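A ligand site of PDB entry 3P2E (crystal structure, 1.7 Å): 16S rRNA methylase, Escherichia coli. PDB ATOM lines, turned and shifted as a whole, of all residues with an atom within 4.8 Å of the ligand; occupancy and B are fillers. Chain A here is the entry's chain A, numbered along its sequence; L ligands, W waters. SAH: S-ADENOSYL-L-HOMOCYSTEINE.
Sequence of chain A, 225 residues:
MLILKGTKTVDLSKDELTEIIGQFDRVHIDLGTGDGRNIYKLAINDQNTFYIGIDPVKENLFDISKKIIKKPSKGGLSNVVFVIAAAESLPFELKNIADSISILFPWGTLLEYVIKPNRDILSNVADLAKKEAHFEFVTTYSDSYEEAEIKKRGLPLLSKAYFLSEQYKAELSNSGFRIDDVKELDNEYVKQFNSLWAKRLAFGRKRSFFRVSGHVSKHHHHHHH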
ATOM      1  N   ASP A  30      20.273   0.256  34.313  1.00  0.00           N
ATOM      2  CA  ASP A  30      20.333   1.589  33.730  1.00  0.00           C
ATOM      3  C   ASP A  30      19.555   1.471  32.425  1.00  0.00           C
ATOM      4  O   ASP A  30      20.015   0.834  31.467  1.00  0.00           O
ATOM      5  CB  ASP A  30      21.783   2.006  33.468  1.00  0.00           C
ATOM      6  CG  ASP A  30      21.899   3.425  32.946  1.00  0.00           C
ATOM      7  OD1 ASP A  30      21.170   4.302  33.460  1.00  0.00           O
ATOM      8  OD2 ASP A  30      22.713   3.666  32.026  1.00  0.00           O
ATOM      9  N   LEU A  31      18.360   2.066  32.407  1.00  0.00           N
ATOM     10  CA  LEU A  31      17.473   2.035  31.235  1.00  0.00           C
ATOM     11  C   LEU A  31      17.777   3.182  30.279  1.00  0.00           C
ATOM     12  O   LEU A  31      17.873   4.329  30.701  1.00  0.00           O
ATOM     13  CB  LEU A  31      16.014   2.104  31.712  1.00  0.00           C
ATOM     14  CG  LEU A  31      14.907   2.139  30.655  1.00  0.00           C
ATOM     15  CD1 LEU A  31      15.015   0.938  29.727  1.00  0.00           C
ATOM     16  CD2 LEU A  31      13.561   2.172  31.361  1.00  0.00           C
ATOM     17  N   GLY A  32      17.903   2.870  28.987  1.00  0.00           N
ATOM     18  CA  GLY A  32      18.249   3.872  27.992  1.00  0.00           C
ATOM     19  C   GLY A  32      19.705   4.217  28.239  1.00  0.00           C
ATOM     20  O   GLY A  32      20.107   5.384  28.198  1.00  0.00           O
ATOM     21  N   THR A  33      20.502   3.186  28.479  1.00  0.00           N
ATOM     22  CA  THR A  33      21.923   3.337  28.807  1.00  0.00           C
ATOM     23  C   THR A  33      22.819   4.026  27.773  1.00  0.00           C
ATOM     24  O   THR A  33      23.875   4.545  28.126  1.00  0.00           O
ATOM     25  CB  THR A  33      22.529   1.961  29.183  1.00  0.00           C
ATOM     26  OG1 THR A  33      23.662   2.156  30.028  1.00  0.00           O
ATOM     27  CG2 THR A  33      22.941   1.186  27.936  1.00  0.00           C
ATOM     28  N   GLY A  34      22.407   4.040  26.519  1.00  0.00           N
ATOM     29  CA  GLY A  34      23.216   4.713  25.513  1.00  0.00           C
ATOM     30  C   GLY A  34      24.455   3.952  25.072  1.00  0.00           C
ATOM     31  O   GLY A  34      24.387   2.760  24.777  1.00  0.00           O
ATOM     32  N   ASN A  38      28.724   5.180  30.719  1.00  0.00           N
ATOM     33  CA  ASN A  38      28.344   5.532  32.082  1.00  0.00           C
ATOM     34  C   ASN A  38      28.318   4.287  32.952  1.00  0.00           C
ATOM     35  O   ASN A  38      28.813   4.285  34.079  1.00  0.00           O
ATOM     36  CB  ASN A  38      26.969   6.209  32.122  1.00  0.00           C
ATOM     37  CG  ASN A  38      26.973   7.587  31.491  1.00  0.00           C
ATOM     38  OD1 ASN A  38      28.010   8.265  31.457  1.00  0.00           O
ATOM     39  ND2 ASN A  38      25.817   8.020  31.001  1.00  0.00           N
ATOM     40  N   ASP A  55      19.172  -0.849  26.223  1.00  0.00           N
ATOM     41  CA  ASP A  55      18.973   0.127  25.146  1.00  0.00           C
ATOM     42  C   ASP A  55      18.550  -0.611  23.880  1.00  0.00           C
ATOM     43  O   ASP A  55      19.068  -1.684  23.564  1.00  0.00           O
ATOM     44  CB  ASP A  55      20.247   0.913  24.861  1.00  0.00           C
ATOM     45  CG  ASP A  55      19.960   2.267  24.231  1.00  0.00           C
ATOM     46  OD1 ASP A  55      20.150   3.289  24.918  1.00  0.00           O
ATOM     47  OD2 ASP A  55      19.505   2.316  23.068  1.00  0.00           O
ATOM     48  N   PRO A  56      17.594  -0.047  23.133  1.00  0.00           N
ATOM     49  CA  PRO A  56      17.121  -0.680  21.895  1.00  0.00           C
ATOM     50  C   PRO A  56      18.100  -0.512  20.728  1.00  0.00           C
ATOM     51  O   PRO A  56      17.959  -1.187  19.711  1.00  0.00           O
ATOM     52  CB  PRO A  56      15.789   0.009  21.638  1.00  0.00           C
ATOM     53  CG  PRO A  56      16.010   1.385  22.204  1.00  0.00           C
ATOM     54  CD  PRO A  56      16.725   1.093  23.502  1.00  0.00           C
ATOM     55  N   VAL A  57      19.065   0.383  20.871  1.00  0.00           N
ATOM     56  CA  VAL A  57      20.055   0.617  19.813  1.00  0.00           C
ATOM     57  C   VAL A  57      21.335  -0.146  20.127  1.00  0.00           C
ATOM     58  O   VAL A  57      22.207   0.334  20.853  1.00  0.00           O
ATOM     59  CB  VAL A  57      20.369   2.128  19.680  1.00  0.00           C
ATOM     60  CG1 VAL A  57      21.439   2.346  18.603  1.00  0.00           C
ATOM     61  CG2 VAL A  57      19.084   2.885  19.334  1.00  0.00           C
ATOM     62  N   ALA A  85      16.665  -3.998  24.454  1.00  0.00           N
ATOM     63  CA  ALA A  85      15.222  -3.937  24.649  1.00  0.00           C
ATOM     64  C   ALA A  85      14.816  -2.491  24.826  1.00  0.00           C
ATOM     65  O   ALA A  85      15.668  -1.620  24.991  1.00  0.00           O
ATOM     66  CB  ALA A  85      14.825  -4.743  25.886  1.00  0.00           C
ATOM     67  N   ALA A  86      13.513  -2.239  24.773  1.00  0.00           N
ATOM     68  CA  ALA A  86      12.965  -0.893  24.943  1.00  0.00           C
ATOM     69  C   ALA A  86      12.041  -0.869  26.159  1.00  0.00           C
ATOM     70  O   ALA A  86      11.561  -1.906  26.596  1.00  0.00           O
ATOM     71  CB  ALA A  86      12.204  -0.482  23.701  1.00  0.00           C
ATOM     72  N   ALA A  87      11.788   0.324  26.685  1.00  0.00           N
ATOM     73  CA  ALA A  87      10.929   0.471  27.845  1.00  0.00           C
ATOM     74  C   ALA A  87       9.524  -0.068  27.622  1.00  0.00           C
ATOM     75  O   ALA A  87       8.864  -0.500  28.573  1.00  0.00           O
ATOM     76  CB  ALA A  87      10.860   1.934  28.270  1.00  0.00           C
ATOM     77  N   GLU A  88       9.070  -0.048  26.373  1.00  0.00           N
ATOM     78  CA  GLU A  88       7.722  -0.537  26.039  1.00  0.00           C
ATOM     79  C   GLU A  88       7.649  -2.068  25.982  1.00  0.00           C
ATOM     80  O   GLU A  88       6.555  -2.628  26.028  1.00  0.00           O
ATOM     81  CB  GLU A  88       7.261   0.030  24.690  1.00  0.00           C
ATOM     82  CG  GLU A  88       7.232   1.541  24.634  1.00  0.00           C
ATOM     83  CD  GLU A  88       8.483   2.135  24.004  1.00  0.00           C
ATOM     84  OE1 GLU A  88       9.595   1.644  24.297  1.00  0.00           O
ATOM     85  OE2 GLU A  88       8.350   3.096  23.219  1.00  0.00           O
ATOM     86  N   LEU A 104      19.121   8.074  32.928  1.00  0.00           N
ATOM     87  CA  LEU A 104      19.964   9.266  32.872  1.00  0.00           C
ATOM     88  C   LEU A 104      19.962   9.989  31.536  1.00  0.00           C
ATOM     89  O   LEU A 104      20.182   9.377  30.497  1.00  0.00           O
ATOM     90  CB  LEU A 104      21.413   8.885  33.205  1.00  0.00           C
ATOM     91  CG  LEU A 104      21.600   7.989  34.431  1.00  0.00           C
ATOM     92  CD1 LEU A 104      23.043   7.520  34.489  1.00  0.00           C
ATOM     93  CD2 LEU A 104      21.220   8.745  35.698  1.00  0.00           C
ATOM     94  N   PHE A 105      19.716  11.298  31.596  1.00  0.00           N
ATOM     95  CA  PHE A 105      19.703  12.146  30.408  1.00  0.00           C
ATOM     96  C   PHE A 105      18.962  11.503  29.239  1.00  0.00           C
ATOM     97  O   PHE A 105      19.488  11.424  28.123  1.00  0.00           O
ATOM     98  CB  PHE A 105      21.147  12.460  30.007  1.00  0.00           C
ATOM     99  CG  PHE A 105      22.030  12.814  31.169  1.00  0.00           C
ATOM    100  CD1 PHE A 105      21.864  14.018  31.846  1.00  0.00           C
ATOM    101  CD2 PHE A 105      22.991  11.914  31.615  1.00  0.00           C
ATOM    102  CE1 PHE A 105      22.637  14.319  32.970  1.00  0.00           C
ATOM    103  CE2 PHE A 105      23.774  12.206  32.739  1.00  0.00           C
ATOM    104  CZ  PHE A 105      23.597  13.419  33.416  1.00  0.00           C
ATOM    105  N   PRO A 106      17.726  11.033  29.485  1.00  0.00           N
ATOM    106  CA  PRO A 106      16.965  10.397  28.410  1.00  0.00           C
ATOM    107  C   PRO A 106      16.629  11.366  27.282  1.00  0.00           C
ATOM    108  O   PRO A 106      16.651  12.583  27.460  1.00  0.00           O
ATOM    109  CB  PRO A 106      15.719   9.882  29.132  1.00  0.00           C
ATOM    110  CG  PRO A 106      15.499  10.928  30.183  1.00  0.00           C
ATOM    111  CD  PRO A 106      16.910  11.162  30.709  1.00  0.00           C
ATOM    112  N   TRP A 107      16.320  10.803  26.121  1.00  0.00           N
ATOM    113  CA  TRP A 107      15.955  11.588  24.950  1.00  0.00           C
ATOM    114  C   TRP A 107      14.912  10.789  24.195  1.00  0.00           C
ATOM    115  O   TRP A 107      14.710   9.601  24.461  1.00  0.00           O
ATOM    116  CB  TRP A 107      17.187  11.817  24.086  1.00  0.00           C
ATOM    117  CG  TRP A 107      17.203  13.134  23.371  1.00  0.00           C
ATOM    118  CD1 TRP A 107      17.220  14.381  23.940  1.00  0.00           C
ATOM    119  CD2 TRP A 107      17.275  13.347  21.951  1.00  0.00           C
ATOM    120  NE1 TRP A 107      17.296  15.349  22.966  1.00  0.00           N
ATOM    121  CE2 TRP A 107      17.334  14.736  21.743  1.00  0.00           C
ATOM    122  CE3 TRP A 107      17.305  12.483  20.842  1.00  0.00           C
ATOM    123  CZ2 TRP A 107      17.409  15.298  20.461  1.00  0.00           C
ATOM    124  CZ3 TRP A 107      17.384  13.049  19.568  1.00  0.00           C
ATOM    125  CH2 TRP A 107      17.435  14.439  19.388  1.00  0.00           C
ATOM    126  N   GLY A 108      14.213  11.418  23.263  1.00  0.00           N
ATOM    127  CA  GLY A 108      13.208  10.685  22.513  1.00  0.00           C
ATOM    128  C   GLY A 108      12.019  10.257  23.343  1.00  0.00           C
ATOM    129  O   GLY A 108      11.603  10.946  24.274  1.00  0.00           O
ATOM    130  N   THR A 109      11.453   9.092  23.011  1.00  0.00           N
ATOM    131  CA  THR A 109      10.282   8.611  23.724  1.00  0.00           C
ATOM    132  C   THR A 109      10.523   8.371  25.213  1.00  0.00           C
ATOM    133  O   THR A 109       9.640   8.615  26.024  1.00  0.00           O
ATOM    134  CB  THR A 109       9.710   7.317  23.077  1.00  0.00           C
ATOM    135  OG1 THR A 109      10.691   6.276  23.125  1.00  0.00           O
ATOM    136  CG2 THR A 109       9.336   7.575  21.635  1.00  0.00           C
ATOM    137  N   LEU A 110      11.717   7.920  25.579  1.00  0.00           N
ATOM    138  CA  LEU A 110      12.008   7.663  26.988  1.00  0.00           C
ATOM    139  C   LEU A 110      11.904   8.937  27.808  1.00  0.00           C
ATOM    140  O   LEU A 110      11.407   8.918  28.941  1.00  0.00           O
ATOM    141  CB  LEU A 110      13.407   7.032  27.150  1.00  0.00           C
ATOM    142  CG  LEU A 110      13.763   6.567  28.570  1.00  0.00           C
ATOM    143  CD1 LEU A 110      12.684   5.622  29.100  1.00  0.00           C
ATOM    144  CD2 LEU A 110      15.116   5.865  28.557  1.00  0.00           C
ATOM    145  N   TYR A 113       8.288   9.602  28.487  1.00  0.00           N
ATOM    146  CA  TYR A 113       7.685   8.681  29.454  1.00  0.00           C
ATOM    147  C   TYR A 113       7.996   9.122  30.875  1.00  0.00           C
ATOM    148  O   TYR A 113       7.194   8.915  31.794  1.00  0.00           O
ATOM    149  CB  TYR A 113       8.199   7.254  29.246  1.00  0.00           C
ATOM    150  CG  TYR A 113       7.837   6.642  27.913  1.00  0.00           C
ATOM    151  CD1 TYR A 113       6.688   7.034  27.240  1.00  0.00           C
ATOM    152  CD2 TYR A 113       8.641   5.659  27.334  1.00  0.00           C
ATOM    153  CE1 TYR A 113       6.336   6.465  26.016  1.00  0.00           C
ATOM    154  CE2 TYR A 113       8.305   5.077  26.121  1.00  0.00           C
ATOM    155  CZ  TYR A 113       7.154   5.487  25.464  1.00  0.00           C
ATOM    156  OH  TYR A 113       6.807   4.923  24.248  1.00  0.00           O
ATOM    157  N   SER A 195      29.719   9.181  29.168  1.00  0.00           N
ATOM    158  CA  SER A 195      29.119   9.032  27.841  1.00  0.00           C
ATOM    159  C   SER A 195      29.382  10.291  27.018  1.00  0.00           C
ATOM    160  O   SER A 195      29.502  11.387  27.559  1.00  0.00           O
ATOM    161  CB  SER A 195      27.608   8.755  27.925  1.00  0.00           C
ATOM    162  OG  SER A 195      26.843   9.935  28.052  1.00  0.00           O
ATOM    163  N   TRP A 197      27.412  11.753  25.067  1.00  0.00           N
ATOM    164  CA  TRP A 197      26.219  12.575  25.193  1.00  0.00           C
ATOM    165  C   TRP A 197      26.275  13.416  26.476  1.00  0.00           C
ATOM    166  O   TRP A 197      26.011  14.620  26.441  1.00  0.00           O
ATOM    167  CB  TRP A 197      24.993  11.654  25.201  1.00  0.00           C
ATOM    168  CG  TRP A 197      23.654  12.268  25.564  1.00  0.00           C
ATOM    169  CD1 TRP A 197      22.822  11.872  26.571  1.00  0.00           C
ATOM    170  CD2 TRP A 197      22.936  13.284  24.835  1.00  0.00           C
ATOM    171  NE1 TRP A 197      21.635  12.564  26.517  1.00  0.00           N
ATOM    172  CE2 TRP A 197      21.680  13.433  25.465  1.00  0.00           C
ATOM    173  CE3 TRP A 197      23.224  14.069  23.718  1.00  0.00           C
ATOM    174  CZ2 TRP A 197      20.717  14.341  25.015  1.00  0.00           C
ATOM    175  CZ3 TRP A 197      22.271  14.977  23.263  1.00  0.00           C
ATOM    176  CH2 TRP A 197      21.024  15.104  23.914  1.00  0.00           C
ATOM    177  N   ALA A 198      26.626  12.791  27.586  1.00  0.00           N
ATOM    178  CA  ALA A 198      26.700  13.523  28.846  1.00  0.00           C
ATOM    179  C   ALA A 198      27.764  14.603  28.791  1.00  0.00           C
ATOM    180  O   ALA A 198      27.572  15.705  29.313  1.00  0.00           O
ATOM    181  CB  ALA A 198      26.986  12.570  30.005  1.00  0.00           C
HETATM  182  N   SAH L   1      21.780   7.354  29.389  1.00  0.00           N
HETATM  183  CA  SAH L   1      22.400   7.777  28.247  1.00  0.00           C
HETATM  184  CB  SAH L   1      21.392   8.426  27.299  1.00  0.00           C
HETATM  185  CG  SAH L   1      21.763   8.564  25.857  1.00  0.00           C
HETATM  186  SD  SAH L   1      20.582   9.308  24.779  1.00  0.00           S
HETATM  187  C   SAH L   1      23.642   8.696  28.651  1.00  0.00           C
HETATM  188  O   SAH L   1      24.409   8.578  27.800  1.00  0.00           O
HETATM  189  OXT SAH L   1      23.713   9.334  29.599  1.00  0.00           O
HETATM  190  C5' SAH L   1      18.933   8.627  25.019  1.00  0.00           C
HETATM  191  C4' SAH L   1      19.041   7.038  24.928  1.00  0.00           C
HETATM  192  O4' SAH L   1      17.717   6.626  25.286  1.00  0.00           O
HETATM  193  C3' SAH L   1      19.337   6.490  23.544  1.00  0.00           C
HETATM  194  O3' SAH L   1      20.515   5.614  23.572  1.00  0.00           O
HETATM  195  C2' SAH L   1      18.008   5.774  23.106  1.00  0.00           C
HETATM  196  O2' SAH L   1      18.140   4.642  22.289  1.00  0.00           O
HETATM  197  C1' SAH L   1      17.349   5.474  24.475  1.00  0.00           C
HETATM  198  N9  SAH L   1      15.841   5.346  24.420  1.00  0.00           N
HETATM  199  C8  SAH L   1      14.942   6.235  23.808  1.00  0.00           C
HETATM  200  N7  SAH L   1      13.691   5.827  23.885  1.00  0.00           N
HETATM  201  C5  SAH L   1      13.819   4.591  24.592  1.00  0.00           C
HETATM  202  C6  SAH L   1      12.756   3.699  24.968  1.00  0.00           C
HETATM  203  N6  SAH L   1      11.458   3.952  24.657  1.00  0.00           N
HETATM  204  N1  SAH L   1      13.167   2.577  25.652  1.00  0.00           N
HETATM  205  C2  SAH L   1      14.501   2.324  25.970  1.00  0.00           C
HETATM  206  N3  SAH L   1      15.529   3.194  25.612  1.00  0.00           N
HETATM  207  C4  SAH L   1      15.093   4.299  24.926  1.00  0.00           C
HETATM  208  O   HOH W   1      12.825   7.576  20.988  1.00  0.00           O
HETATM  209  O   HOH W   2      25.193   7.462  25.239  1.00  0.00           O
HETATM  210  O   HOH W   3      15.910   4.833  20.785  1.00  0.00           O
HETATM  211  O   HOH W   4      20.075   5.873  31.370  1.00  0.00           O
HETATM  212  O   HOH W   5      23.781   5.770  30.672  1.00  0.00           O
HETATM  213  O   HOH W   6      22.467   4.845  21.826  1.00  0.00           O
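OD1 of Asp 55 lies within hydrogen-bond range of O3' of the ligand (2.7 Å).
The side-chain hydroxyl of Ser 195 lies within hydrogen-bond range of an oxygen (O) of the ligand, 2.8 Å away.
N of the ligand lies within hydrogen-bond range of O of Leu 104, at 2.8 Å.
N1 of the ligand lies within hydrogen-bond range of N of Ala 87 (2.8 Å).
O of Gly 32 sits at hydrogen-bond distance from N of the ligand (2.8 Å).
An oxygen (OXT) of the ligand sits at hydrogen-bond distance from the side-chain amide nitrogen of Asn 38 (2.8 Å).
The side-chain hydroxyl of Thr 109 lies within hydrogen-bond range of a nitrogen (N6) of the ligand (2.9 Å).
OE1 of Glu 88 lies within hydrogen-bond range of N6 of the ligand, 3.0 Å away.
A nitrogen (N7) of the ligand sits at hydrogen-bond distance from the backbone NH (N) of Leu 110 (3.3 Å).
Water W5 lies within hydrogen-bond range of the side-chain carboxylate (OD2) of Asp 30 (2.7 Å), the backbone carbonyl oxygen (O) of Thr 33 (2.8 Å), a nitrogen (N) of the ligand (2.9 Å) and the side-chain amide nitrogen (ND2) of Asn 38 (3.1 Å).
Water W1 lies within hydrogen-bond range of N of Thr 109 (2.9 Å) and N7 of the ligand (3.5 Å).
The side-chain carboxylate (OD1) of Asp 55 sits at hydrogen-bond distance from the backbone NH (N) of Gly 34, 2.9 Å away.
The side-chain carboxylate (OD2) of Asp 55 lies within hydrogen-bond range of the backbone NH (N) of Val 57, 3.0 Å away.
The backbone carbonyl oxygen of Asp 55 lies within hydrogen-bond range of the backbone NH of Ala 85, at 3.5 Å.
N of Ser 195 sits at hydrogen-bond distance from OD1 of Asn 38 (3.0 Å).
OG of Ser 195 sits at hydrogen-bond distance from N of Ala 198 (2.9 Å).
The side-chain hydroxyl (OH) of Tyr 113 lies within hydrogen-bond range of the side-chain carboxylate (OE2) of Glu 88, 2.6 Å away.
The backbone carbonyl oxygen (O) of Phe 105 sits at hydrogen-bond distance from the indole nitrogen (NE1) of Trp 197.
The side-chain carboxylate of Asp 30 is in hydrogen-bond range of the side-chain hydroxyl of Thr 33 (2.7 Å).
Thr 33 touches the ligand (O to CA, 3.6 Å).
Gly 34 touches the ligand (CA to O3', 3.4 Å).
Pro 56 touches the ligand.
Val 57 touches the ligand.
Ala 86 touches the ligand.
Phe 105 touches the ligand.
O of Trp 107 touches C8 of the ligand, 3.4 Å away.
CE2 of Tyr 113 touches N6 of the ligand (3.7 Å).
Trp 197 touches the ligand.
Hydrophobic or aromatic side chains that line the ligand: Pro 56, Val 57, Ala 86, Ala 87, Phe 105, Trp 107, Leu 110, Tyr 113 and Trp 197.
Along chain A the residues within 4 Å of the ligand span positions 32 to 197.
The nearest printed residue that does not touch the ligand is Leu 31 (4.04 Å).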
